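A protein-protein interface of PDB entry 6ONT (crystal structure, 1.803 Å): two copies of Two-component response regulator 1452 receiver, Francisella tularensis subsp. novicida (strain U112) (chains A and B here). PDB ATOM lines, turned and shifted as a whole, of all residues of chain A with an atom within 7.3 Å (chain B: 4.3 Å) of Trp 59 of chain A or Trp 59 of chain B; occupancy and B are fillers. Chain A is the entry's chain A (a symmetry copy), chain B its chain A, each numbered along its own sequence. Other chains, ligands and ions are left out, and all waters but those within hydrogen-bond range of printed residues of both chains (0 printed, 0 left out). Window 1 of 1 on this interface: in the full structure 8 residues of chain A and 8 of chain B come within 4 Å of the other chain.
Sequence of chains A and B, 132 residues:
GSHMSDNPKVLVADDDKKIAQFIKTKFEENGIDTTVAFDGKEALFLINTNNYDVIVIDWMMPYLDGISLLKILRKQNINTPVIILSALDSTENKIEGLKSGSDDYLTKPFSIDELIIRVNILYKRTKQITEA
The backbone carbonyl oxygen of Leu 88 of chain A sits at hydrogen-bond distance from the side-chain hydroxyl of Tyr 105 of chain A, at 2.7 Å. N of Gly 66 of chain B lies within hydrogen-bond range of O of Trp 59 of chain B (3.0 Å). OG of Ser 86 of chain B sits at hydrogen-bond distance from N of Leu 88 of chain B (2.9 Å). The backbone carbonyl oxygen (O) of Trp 59 of chain A lies within hydrogen-bond range of the backbone NH (N) of Gly 66 of chain A (3.0 Å). N of Trp 59 of chain A sits at hydrogen-bond distance from O of Leu 85 of chain A, at 2.9 Å. The side-chain hydroxyl (OG) of Ser 86 of chain A lies within hydrogen-bond range of the backbone NH (N) of Leu 88 of chain A, at 2.9 Å.
Trp 59 of chain B touches Trp 59 of chain A. Trp 59 of chain A touches Leu 88 of chain B. Trp 59 of chain B touches Leu 88 of chain A.
Of chain B, only Trp 59 (3.9 Å) and Leu 88 (3.9 Å) come within 4 Å of Trp 59 of chain A. Printed residues of chain A within 4 Å of Trp 59 of chain B: Trp 59 (3.9 Å) and Leu 88 (3.9 Å). Of the printed residues of chain B, Leu 88 of chain A touches Trp 59 (3.9 Å). Of the printed residues of chain A, Leu 88 of chain B touches Trp 59 (3.9 Å). The nearest printed residue of chain B that does not touch Trp 59 of chain A is Met 60 of chain B (6.5 Å). The nearest residue of chain A that does not touch Trp 59 of chain B is Met 60 of chain A (6.5 Å).
Hydrophobic or aromatic side chains of chain B within 4 Å of the printed part of chain A: Trp 59 and Leu 88. Of the 20 printed residues of chain A, 2 touch a printed residue of chain B. Printed residues of chain A that touch a printed residue of chain B: Trp 59 and Leu 88. Among the printed residues, no Asp or Glu carboxylate lies within 4 Å of a Lys or Arg side-chain nitrogen of the other chain.
Trp 59 of chain A touches its own counterpart, Trp 59 of chain B. Trp 59 of chain A touches Leu 88 of chain B, and with the chains exchanged Leu 88 of chain A touches Trp 59 of chain B. Of the 3 pairs that touch across the chains among the printed residues, 3 have their exchanged pair printed and touching as well.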
ATOM      1  N   ALA A  13      -7.159  -2.979 -13.475  1.00  0.00           N
ATOM      2  CA  ALA A  13      -5.981  -2.423 -14.135  1.00  0.00           C
ATOM      3  C   ALA A  13      -6.007  -2.768 -15.620  1.00  0.00           C
ATOM      4  O   ALA A  13      -5.892  -3.938 -15.993  1.00  0.00           O
ATOM      5  CB  ALA A  13      -4.703  -2.943 -13.480  1.00  0.00           C
ATOM      6  N   ASP A  14      -6.162  -1.748 -16.462  1.00  0.00           N
ATOM      7  CA  ASP A  14      -5.930  -1.892 -17.892  1.00  0.00           C
ATOM      8  C   ASP A  14      -5.580  -0.529 -18.472  1.00  0.00           C
ATOM      9  O   ASP A  14      -6.073   0.501 -18.009  1.00  0.00           O
ATOM     10  CB  ASP A  14      -7.143  -2.482 -18.618  1.00  0.00           C
ATOM     11  CG  ASP A  14      -6.796  -2.942 -20.025  1.00  0.00           C
ATOM     12  OD1 ASP A  14      -5.586  -3.001 -20.346  1.00  0.00           O
ATOM     13  OD2 ASP A  14      -7.720  -3.233 -20.813  1.00  0.00           O
ATOM     14  N   ASP A  15      -4.746  -0.529 -19.512  1.00  0.00           N
ATOM     15  CA  ASP A  15      -4.390   0.715 -20.183  1.00  0.00           C
ATOM     16  C   ASP A  15      -5.376   1.112 -21.278  1.00  0.00           C
ATOM     17  O   ASP A  15      -5.293   2.237 -21.777  1.00  0.00           O
ATOM     18  CB  ASP A  15      -2.968   0.622 -20.760  1.00  0.00           C
ATOM     19  CG  ASP A  15      -2.801  -0.517 -21.759  1.00  0.00           C
ATOM     20  OD1 ASP A  15      -3.504  -1.537 -21.622  1.00  0.00           O
ATOM     21  OD2 ASP A  15      -1.960  -0.404 -22.677  1.00  0.00           O
ATOM     22  N   ILE A  57      -6.805  -7.809 -13.521  1.00  0.00           N
ATOM     23  CA  ILE A  57      -5.570  -7.351 -14.144  1.00  0.00           C
ATOM     24  C   ILE A  57      -5.560  -7.736 -15.616  1.00  0.00           C
ATOM     25  O   ILE A  57      -5.732  -8.914 -15.957  1.00  0.00           O
ATOM     26  CB  ILE A  57      -4.333  -7.941 -13.443  1.00  0.00           C
ATOM     27  CG1 ILE A  57      -4.344  -7.640 -11.944  1.00  0.00           C
ATOM     28  CG2 ILE A  57      -3.074  -7.405 -14.103  1.00  0.00           C
ATOM     29  CD1 ILE A  57      -3.163  -8.274 -11.221  1.00  0.00           C
ATOM     30  N   ASP A  58      -5.332  -6.746 -16.484  1.00  0.00           N
ATOM     31  CA  ASP A  58      -5.146  -7.010 -17.905  1.00  0.00           C
ATOM     32  C   ASP A  58      -3.740  -7.526 -18.179  1.00  0.00           C
ATOM     33  O   ASP A  58      -2.776  -7.169 -17.498  1.00  0.00           O
ATOM     34  CB  ASP A  58      -5.411  -5.752 -18.729  1.00  0.00           C
ATOM     35  CG  ASP A  58      -5.361  -6.024 -20.225  1.00  0.00           C
ATOM     36  OD1 ASP A  58      -4.361  -5.663 -20.891  1.00  0.00           O
ATOM     37  OD2 ASP A  58      -6.312  -6.650 -20.724  1.00  0.00           O
ATOM     38  N   TRP A  59      -3.626  -8.366 -19.217  1.00  0.00           N
ATOM     39  CA  TRP A  59      -2.383  -9.096 -19.446  1.00  0.00           C
ATOM     40  C   TRP A  59      -1.261  -8.195 -19.930  1.00  0.00           C
ATOM     41  O   TRP A  59      -0.086  -8.517 -19.725  1.00  0.00           O
ATOM     42  CB  TRP A  59      -2.596 -10.226 -20.459  1.00  0.00           C
ATOM     43  CG  TRP A  59      -2.798  -9.749 -21.850  1.00  0.00           C
ATOM     44  CD1 TRP A  59      -3.853  -9.024 -22.329  1.00  0.00           C
ATOM     45  CD2 TRP A  59      -1.911  -9.937 -22.957  1.00  0.00           C
ATOM     46  NE1 TRP A  59      -3.674  -8.752 -23.662  1.00  0.00           N
ATOM     47  CE2 TRP A  59      -2.488  -9.301 -24.070  1.00  0.00           C
ATOM     48  CE3 TRP A  59      -0.676 -10.573 -23.112  1.00  0.00           C
ATOM     49  CZ2 TRP A  59      -1.880  -9.288 -25.324  1.00  0.00           C
ATOM     50  CZ3 TRP A  59      -0.079 -10.560 -24.367  1.00  0.00           C
ATOM     51  CH2 TRP A  59      -0.685  -9.925 -25.452  1.00  0.00           C
ATOM     52  N   MET A  60      -1.583  -7.072 -20.571  1.00  0.00           N
ATOM     53  CA  MET A  60      -0.546  -6.210 -21.128  1.00  0.00           C
ATOM     54  C   MET A  60      -0.847  -4.745 -20.860  1.00  0.00           C
ATOM     55  O   MET A  60      -1.866  -4.215 -21.313  1.00  0.00           O
ATOM     56  CB  MET A  60      -0.409  -6.474 -22.628  1.00  0.00           C
ATOM     57  CG  MET A  60       0.818  -5.826 -23.286  1.00  0.00           C
ATOM     58  SD  MET A  60       2.403  -6.096 -22.449  1.00  0.00           S
ATOM     59  CE  MET A  60       2.432  -7.884 -22.410  1.00  0.00           C
ATOM     60  N   MET A  61       0.079  -4.091 -20.163  1.00  0.00           N
ATOM     61  CA  MET A  61      -0.006  -2.670 -19.867  1.00  0.00           C
ATOM     62  C   MET A  61       1.406  -2.114 -19.753  1.00  0.00           C
ATOM     63  O   MET A  61       2.367  -2.873 -19.602  1.00  0.00           O
ATOM     64  CB  MET A  61      -0.750  -2.407 -18.556  1.00  0.00           C
ATOM     65  CG  MET A  61      -1.842  -3.362 -18.192  1.00  0.00           C
ATOM     66  SD  MET A  61      -2.392  -2.949 -16.521  1.00  0.00           S
ATOM     67  CE  MET A  61      -1.544  -4.161 -15.514  1.00  0.00           C
ATOM     68  N   LEU A  64       4.506  -2.616 -16.164  1.00  0.00           N
ATOM     69  CA  LEU A  64       4.428  -3.994 -15.701  1.00  0.00           C
ATOM     70  C   LEU A  64       3.238  -4.665 -16.366  1.00  0.00           C
ATOM     71  O   LEU A  64       2.097  -4.223 -16.192  1.00  0.00           O
ATOM     72  CB  LEU A  64       4.294  -4.063 -14.179  1.00  0.00           C
ATOM     73  CG  LEU A  64       5.487  -4.017 -13.229  1.00  0.00           C
ATOM     74  CD1 LEU A  64       4.964  -4.038 -11.800  1.00  0.00           C
ATOM     75  CD2 LEU A  64       6.391  -5.192 -13.458  1.00  0.00           C
ATOM     76  N   ASP A  65       3.514  -5.704 -17.153  1.00  0.00           N
ATOM     77  CA  ASP A  65       2.446  -6.531 -17.693  1.00  0.00           C
ATOM     78  C   ASP A  65       1.748  -7.283 -16.557  1.00  0.00           C
ATOM     79  O   ASP A  65       2.253  -7.384 -15.434  1.00  0.00           O
ATOM     80  CB  ASP A  65       2.985  -7.506 -18.737  1.00  0.00           C
ATOM     81  CG  ASP A  65       3.946  -8.496 -18.158  1.00  0.00           C
ATOM     82  OD1 ASP A  65       3.497  -9.595 -17.776  1.00  0.00           O
ATOM     83  OD2 ASP A  65       5.141  -8.163 -18.059  1.00  0.00           O
ATOM     84  N   GLY A  66       0.563  -7.814 -16.864  1.00  0.00           N
ATOM     85  CA  GLY A  66      -0.286  -8.357 -15.815  1.00  0.00           C
ATOM     86  C   GLY A  66       0.318  -9.552 -15.105  1.00  0.00           C
ATOM     87  O   GLY A  66       0.266  -9.646 -13.876  1.00  0.00           O
ATOM     88  N   ILE A  67       0.903 -10.478 -15.860  1.00  0.00           N
ATOM     89  CA  ILE A  67       1.482 -11.663 -15.237  1.00  0.00           C
ATOM     90  C   ILE A  67       2.683 -11.284 -14.378  1.00  0.00           C
ATOM     91  O   ILE A  67       2.903 -11.857 -13.304  1.00  0.00           O
ATOM     92  CB  ILE A  67       1.868 -12.701 -16.308  1.00  0.00           C
ATOM     93  CG1 ILE A  67       0.611 -13.248 -16.975  1.00  0.00           C
ATOM     94  CG2 ILE A  67       2.737 -13.781 -15.691  1.00  0.00           C
ATOM     95  CD1 ILE A  67      -0.201 -14.135 -16.080  1.00  0.00           C
ATOM     96  N   SER A  68       3.482 -10.316 -14.832  1.00  0.00           N
ATOM     97  CA  SER A  68       4.637  -9.887 -14.048  1.00  0.00           C
ATOM     98  C   SER A  68       4.200  -9.222 -12.748  1.00  0.00           C
ATOM     99  O   SER A  68       4.803  -9.457 -11.688  1.00  0.00           O
ATOM    100  CB  SER A  68       5.502  -8.925 -14.863  1.00  0.00           C
ATOM    101  OG  SER A  68       6.187  -9.579 -15.918  1.00  0.00           O
ATOM    102  N   ILE A  84      -7.166 -12.594 -14.102  1.00  0.00           N
ATOM    103  CA  ILE A  84      -6.410 -12.117 -15.253  1.00  0.00           C
ATOM    104  C   ILE A  84      -7.335 -12.065 -16.463  1.00  0.00           C
ATOM    105  O   ILE A  84      -8.115 -12.993 -16.709  1.00  0.00           O
ATOM    106  CB  ILE A  84      -5.195 -13.019 -15.539  1.00  0.00           C
ATOM    107  CG1 ILE A  84      -4.110 -12.839 -14.477  1.00  0.00           C
ATOM    108  CG2 ILE A  84      -4.627 -12.698 -16.919  1.00  0.00           C
ATOM    109  CD1 ILE A  84      -3.052 -13.934 -14.513  1.00  0.00           C
ATOM    110  N   LEU A  85      -7.256 -10.969 -17.211  1.00  0.00           N
ATOM    111  CA  LEU A  85      -7.908 -10.845 -18.511  1.00  0.00           C
ATOM    112  C   LEU A  85      -6.820 -10.890 -19.572  1.00  0.00           C
ATOM    113  O   LEU A  85      -5.924 -10.040 -19.570  1.00  0.00           O
ATOM    114  CB  LEU A  85      -8.696  -9.542 -18.622  1.00  0.00           C
ATOM    115  CG  LEU A  85      -9.675  -9.226 -17.497  1.00  0.00           C
ATOM    116  CD1 LEU A  85     -10.304  -7.849 -17.747  1.00  0.00           C
ATOM    117  CD2 LEU A  85     -10.746 -10.304 -17.337  1.00  0.00           C
ATOM    118  N   SER A  86      -6.884 -11.864 -20.474  1.00  0.00           N
ATOM    119  CA  SER A  86      -5.766 -12.052 -21.390  1.00  0.00           C
ATOM    120  C   SER A  86      -6.215 -12.364 -22.806  1.00  0.00           C
ATOM    121  O   SER A  86      -7.205 -13.070 -23.020  1.00  0.00           O
ATOM    122  CB  SER A  86      -4.846 -13.175 -20.883  1.00  0.00           C
ATOM    123  OG  SER A  86      -3.783 -13.420 -21.786  1.00  0.00           O
ATOM    124  N   ALA A  87      -5.444 -11.858 -23.775  1.00  0.00           N
ATOM    125  CA  ALA A  87      -5.612 -12.211 -25.178  1.00  0.00           C
ATOM    126  C   ALA A  87      -4.969 -13.545 -25.520  1.00  0.00           C
ATOM    127  O   ALA A  87      -5.215 -14.074 -26.607  1.00  0.00           O
ATOM    128  CB  ALA A  87      -5.019 -11.120 -26.072  1.00  0.00           C
ATOM    129  N   LEU A  88      -4.153 -14.095 -24.626  1.00  0.00           N
ATOM    130  CA  LEU A  88      -3.530 -15.400 -24.838  1.00  0.00           C
ATOM    131  C   LEU A  88      -4.533 -16.470 -24.425  1.00  0.00           C
ATOM    132  O   LEU A  88      -4.729 -16.732 -23.234  1.00  0.00           O
ATOM    133  CB  LEU A  88      -2.242 -15.507 -24.036  1.00  0.00           C
ATOM    134  CG  LEU A  88      -1.189 -14.438 -24.341  1.00  0.00           C
ATOM    135  CD1 LEU A  88       0.044 -14.613 -23.454  1.00  0.00           C
ATOM    136  CD2 LEU A  88      -0.803 -14.470 -25.817  1.00  0.00           C
ATOM    137  N   TYR A 105      -8.874 -16.801 -14.974  1.00  0.00           N
ATOM    138  CA  TYR A 105      -8.160 -16.422 -16.191  1.00  0.00           C
ATOM    139  C   TYR A 105      -9.230 -16.386 -17.275  1.00  0.00           C
ATOM    140  O   TYR A 105      -9.787 -17.430 -17.631  1.00  0.00           O
ATOM    141  CB  TYR A 105      -7.052 -17.430 -16.491  1.00  0.00           C
ATOM    142  CG  TYR A 105      -6.132 -17.077 -17.641  1.00  0.00           C
ATOM    143  CD1 TYR A 105      -6.530 -17.289 -18.953  1.00  0.00           C
ATOM    144  CD2 TYR A 105      -4.852 -16.564 -17.420  1.00  0.00           C
ATOM    145  CE1 TYR A 105      -5.699 -16.984 -20.013  1.00  0.00           C
ATOM    146  CE2 TYR A 105      -4.015 -16.259 -18.481  1.00  0.00           C
ATOM    147  CZ  TYR A 105      -4.446 -16.469 -19.774  1.00  0.00           C
ATOM    148  OH  TYR A 105      -3.617 -16.177 -20.828  1.00  0.00           O
ATOM    149  N   LYS A 108      -9.969 -12.971 -23.807  1.00  0.00           N
ATOM    150  CA  LYS A 108     -10.637 -11.871 -24.489  1.00  0.00           C
ATOM    151  C   LYS A 108     -10.997 -12.280 -25.917  1.00  0.00           C
ATOM    152  O   LYS A 108     -10.218 -12.974 -26.576  1.00  0.00           O
ATOM    153  CB  LYS A 108      -9.736 -10.640 -24.513  1.00  0.00           C
ATOM    154  CG  LYS A 108      -9.207 -10.251 -23.140  1.00  0.00           C
ATOM    155  CD  LYS A 108      -7.968  -9.373 -23.252  1.00  0.00           C
ATOM    156  CE  LYS A 108      -8.193  -7.990 -22.688  1.00  0.00           C
ATOM    157  NZ  LYS A 108      -7.404  -6.956 -23.419  1.00  0.00           N
ATOM    158  N   ILE B  57      12.552 -16.380 -34.354  1.00  0.00           N
ATOM    159  CA  ILE B  57      11.613 -16.963 -33.404  1.00  0.00           C
ATOM    160  C   ILE B  57      10.391 -16.066 -33.268  1.00  0.00           C
ATOM    161  O   ILE B  57      10.520 -14.870 -32.975  1.00  0.00           O
ATOM    162  CB  ILE B  57      12.264 -17.169 -32.024  1.00  0.00           C
ATOM    163  CG1 ILE B  57      13.540 -18.004 -32.127  1.00  0.00           C
ATOM    164  CG2 ILE B  57      11.259 -17.812 -31.083  1.00  0.00           C
ATOM    165  CD1 ILE B  57      14.235 -18.161 -30.782  1.00  0.00           C
ATOM    166  N   ASP B  58       9.204 -16.652 -33.457  1.00  0.00           N
ATOM    167  CA  ASP B  58       7.958 -15.941 -33.205  1.00  0.00           C
ATOM    168  C   ASP B  58       7.656 -15.891 -31.714  1.00  0.00           C
ATOM    169  O   ASP B  58       7.999 -16.799 -30.954  1.00  0.00           O
ATOM    170  CB  ASP B  58       6.799 -16.598 -33.952  1.00  0.00           C
ATOM    171  CG  ASP B  58       5.508 -15.803 -33.824  1.00  0.00           C
ATOM    172  OD1 ASP B  58       4.604 -16.204 -33.053  1.00  0.00           O
ATOM    173  OD2 ASP B  58       5.426 -14.741 -34.464  1.00  0.00           O
ATOM    174  N   TRP B  59       6.978 -14.813 -31.299  1.00  0.00           N
ATOM    175  CA  TRP B  59       6.819 -14.540 -29.873  1.00  0.00           C
ATOM    176  C   TRP B  59       5.871 -15.514 -29.198  1.00  0.00           C
ATOM    177  O   TRP B  59       5.980 -15.734 -27.987  1.00  0.00           O
ATOM    178  CB  TRP B  59       6.319 -13.109 -29.647  1.00  0.00           C
ATOM    179  CG  TRP B  59       4.903 -12.903 -30.041  1.00  0.00           C
ATOM    180  CD1 TRP B  59       4.380 -12.963 -31.301  1.00  0.00           C
ATOM    181  CD2 TRP B  59       3.803 -12.626 -29.167  1.00  0.00           C
ATOM    182  NE1 TRP B  59       3.026 -12.739 -31.264  1.00  0.00           N
ATOM    183  CE2 TRP B  59       2.649 -12.531 -29.964  1.00  0.00           C
ATOM    184  CE3 TRP B  59       3.681 -12.459 -27.785  1.00  0.00           C
ATOM    185  CZ2 TRP B  59       1.389 -12.269 -29.429  1.00  0.00           C
ATOM    186  CZ3 TRP B  59       2.423 -12.193 -27.260  1.00  0.00           C
ATOM    187  CH2 TRP B  59       1.299 -12.098 -28.083  1.00  0.00           C
ATOM    188  N   MET B  60       4.938 -16.107 -29.941  1.00  0.00           N
ATOM    189  CA  MET B  60       3.951 -16.990 -29.329  1.00  0.00           C
ATOM    190  C   MET B  60       3.730 -18.236 -30.171  1.00  0.00           C
ATOM    191  O   MET B  60       3.294 -18.152 -31.324  1.00  0.00           O
ATOM    192  CB  MET B  60       2.638 -16.231 -29.124  1.00  0.00           C
ATOM    193  CG  MET B  60       1.603 -16.960 -28.256  1.00  0.00           C
ATOM    194  SD  MET B  60       2.208 -17.614 -26.678  1.00  0.00           S
ATOM    195  CE  MET B  60       2.869 -16.117 -25.956  1.00  0.00           C
ATOM    196  N   ASP B  65       6.766 -20.396 -25.723  1.00  0.00           N
ATOM    197  CA  ASP B  65       6.736 -19.107 -26.394  1.00  0.00           C
ATOM    198  C   ASP B  65       8.162 -18.661 -26.727  1.00  0.00           C
ATOM    199  O   ASP B  65       9.150 -19.190 -26.204  1.00  0.00           O
ATOM    200  CB  ASP B  65       6.029 -18.060 -25.535  1.00  0.00           C
ATOM    201  CG  ASP B  65       6.754 -17.781 -24.256  1.00  0.00           C
ATOM    202  OD1 ASP B  65       7.567 -16.836 -24.236  1.00  0.00           O
ATOM    203  OD2 ASP B  65       6.530 -18.525 -23.283  1.00  0.00           O
ATOM    204  N   GLY B  66       8.262 -17.673 -27.617  1.00  0.00           N
ATOM    205  CA  GLY B  66       9.559 -17.319 -28.171  1.00  0.00           C
ATOM    206  C   GLY B  66      10.535 -16.791 -27.139  1.00  0.00           C
ATOM    207  O   GLY B  66      11.709 -17.169 -27.131  1.00  0.00           O
ATOM    208  N   LEU B  85      10.339 -12.096 -33.601  1.00  0.00           N
ATOM    209  CA  LEU B  85       9.206 -11.467 -34.270  1.00  0.00           C
ATOM    210  C   LEU B  85       8.065 -11.400 -33.267  1.00  0.00           C
ATOM    211  O   LEU B  85       7.620 -12.440 -32.771  1.00  0.00           O
ATOM    212  CB  LEU B  85       8.774 -12.256 -35.503  1.00  0.00           C
ATOM    213  CG  LEU B  85       9.860 -12.617 -36.510  1.00  0.00           C
ATOM    214  CD1 LEU B  85       9.248 -13.470 -37.629  1.00  0.00           C
ATOM    215  CD2 LEU B  85      10.563 -11.383 -37.075  1.00  0.00           C
ATOM    216  N   SER B  86       7.588 -10.198 -32.961  1.00  0.00           N
ATOM    217  CA  SER B  86       6.627 -10.075 -31.873  1.00  0.00           C
ATOM    218  C   SER B  86       5.505  -9.101 -32.188  1.00  0.00           C
ATOM    219  O   SER B  86       5.719  -8.068 -32.829  1.00  0.00           O
ATOM    220  CB  SER B  86       7.338  -9.641 -30.581  1.00  0.00           C
ATOM    221  OG  SER B  86       6.418  -9.456 -29.521  1.00  0.00           O
ATOM    222  N   ALA B  87       4.307  -9.428 -31.689  1.00  0.00           N
ATOM    223  CA  ALA B  87       3.167  -8.522 -31.729  1.00  0.00           C
ATOM    224  C   ALA B  87       3.216  -7.480 -30.624  1.00  0.00           C
ATOM    225  O   ALA B  87       2.442  -6.521 -30.662  1.00  0.00           O
ATOM    226  CB  ALA B  87       1.862  -9.313 -31.620  1.00  0.00           C
ATOM    227  N   LEU B  88       4.100  -7.647 -29.644  1.00  0.00           N
ATOM    228  CA  LEU B  88       4.262  -6.673 -28.567  1.00  0.00           C
ATOM    229  C   LEU B  88       5.184  -5.570 -29.068  1.00  0.00           C
ATOM    230  O   LEU B  88       6.406  -5.740 -29.128  1.00  0.00           O
ATOM    231  CB  LEU B  88       4.827  -7.348 -27.325  1.00  0.00           C
ATOM    232  CG  LEU B  88       3.996  -8.510 -26.775  1.00  0.00           C
ATOM    233  CD1 LEU B  88       4.672  -9.141 -25.558  1.00  0.00           C
ATOM    234  CD2 LEU B  88       2.584  -8.046 -26.431  1.00  0.00           C
ATOM    235  N   LYS B 108       5.414  -6.873 -35.426  1.00  0.00           N
ATOM    236  CA  LYS B 108       4.508  -7.309 -36.480  1.00  0.00           C
ATOM    237  C   LYS B 108       3.396  -6.279 -36.676  1.00  0.00           C
ATOM    238  O   LYS B 108       2.906  -5.707 -35.698  1.00  0.00           O
ATOM    239  CB  LYS B 108       3.905  -8.665 -36.128  1.00  0.00           C
ATOM    240  CG  LYS B 108       4.945  -9.716 -35.771  1.00  0.00           C
ATOM    241  CD  LYS B 108       4.329 -10.856 -34.972  1.00  0.00           C
ATOM    242  CE  LYS B 108       4.398 -12.174 -35.707  1.00  0.00           C
ATOM    243  NZ  LYS B 108       3.230 -13.049 -35.394  1.00  0.00           N
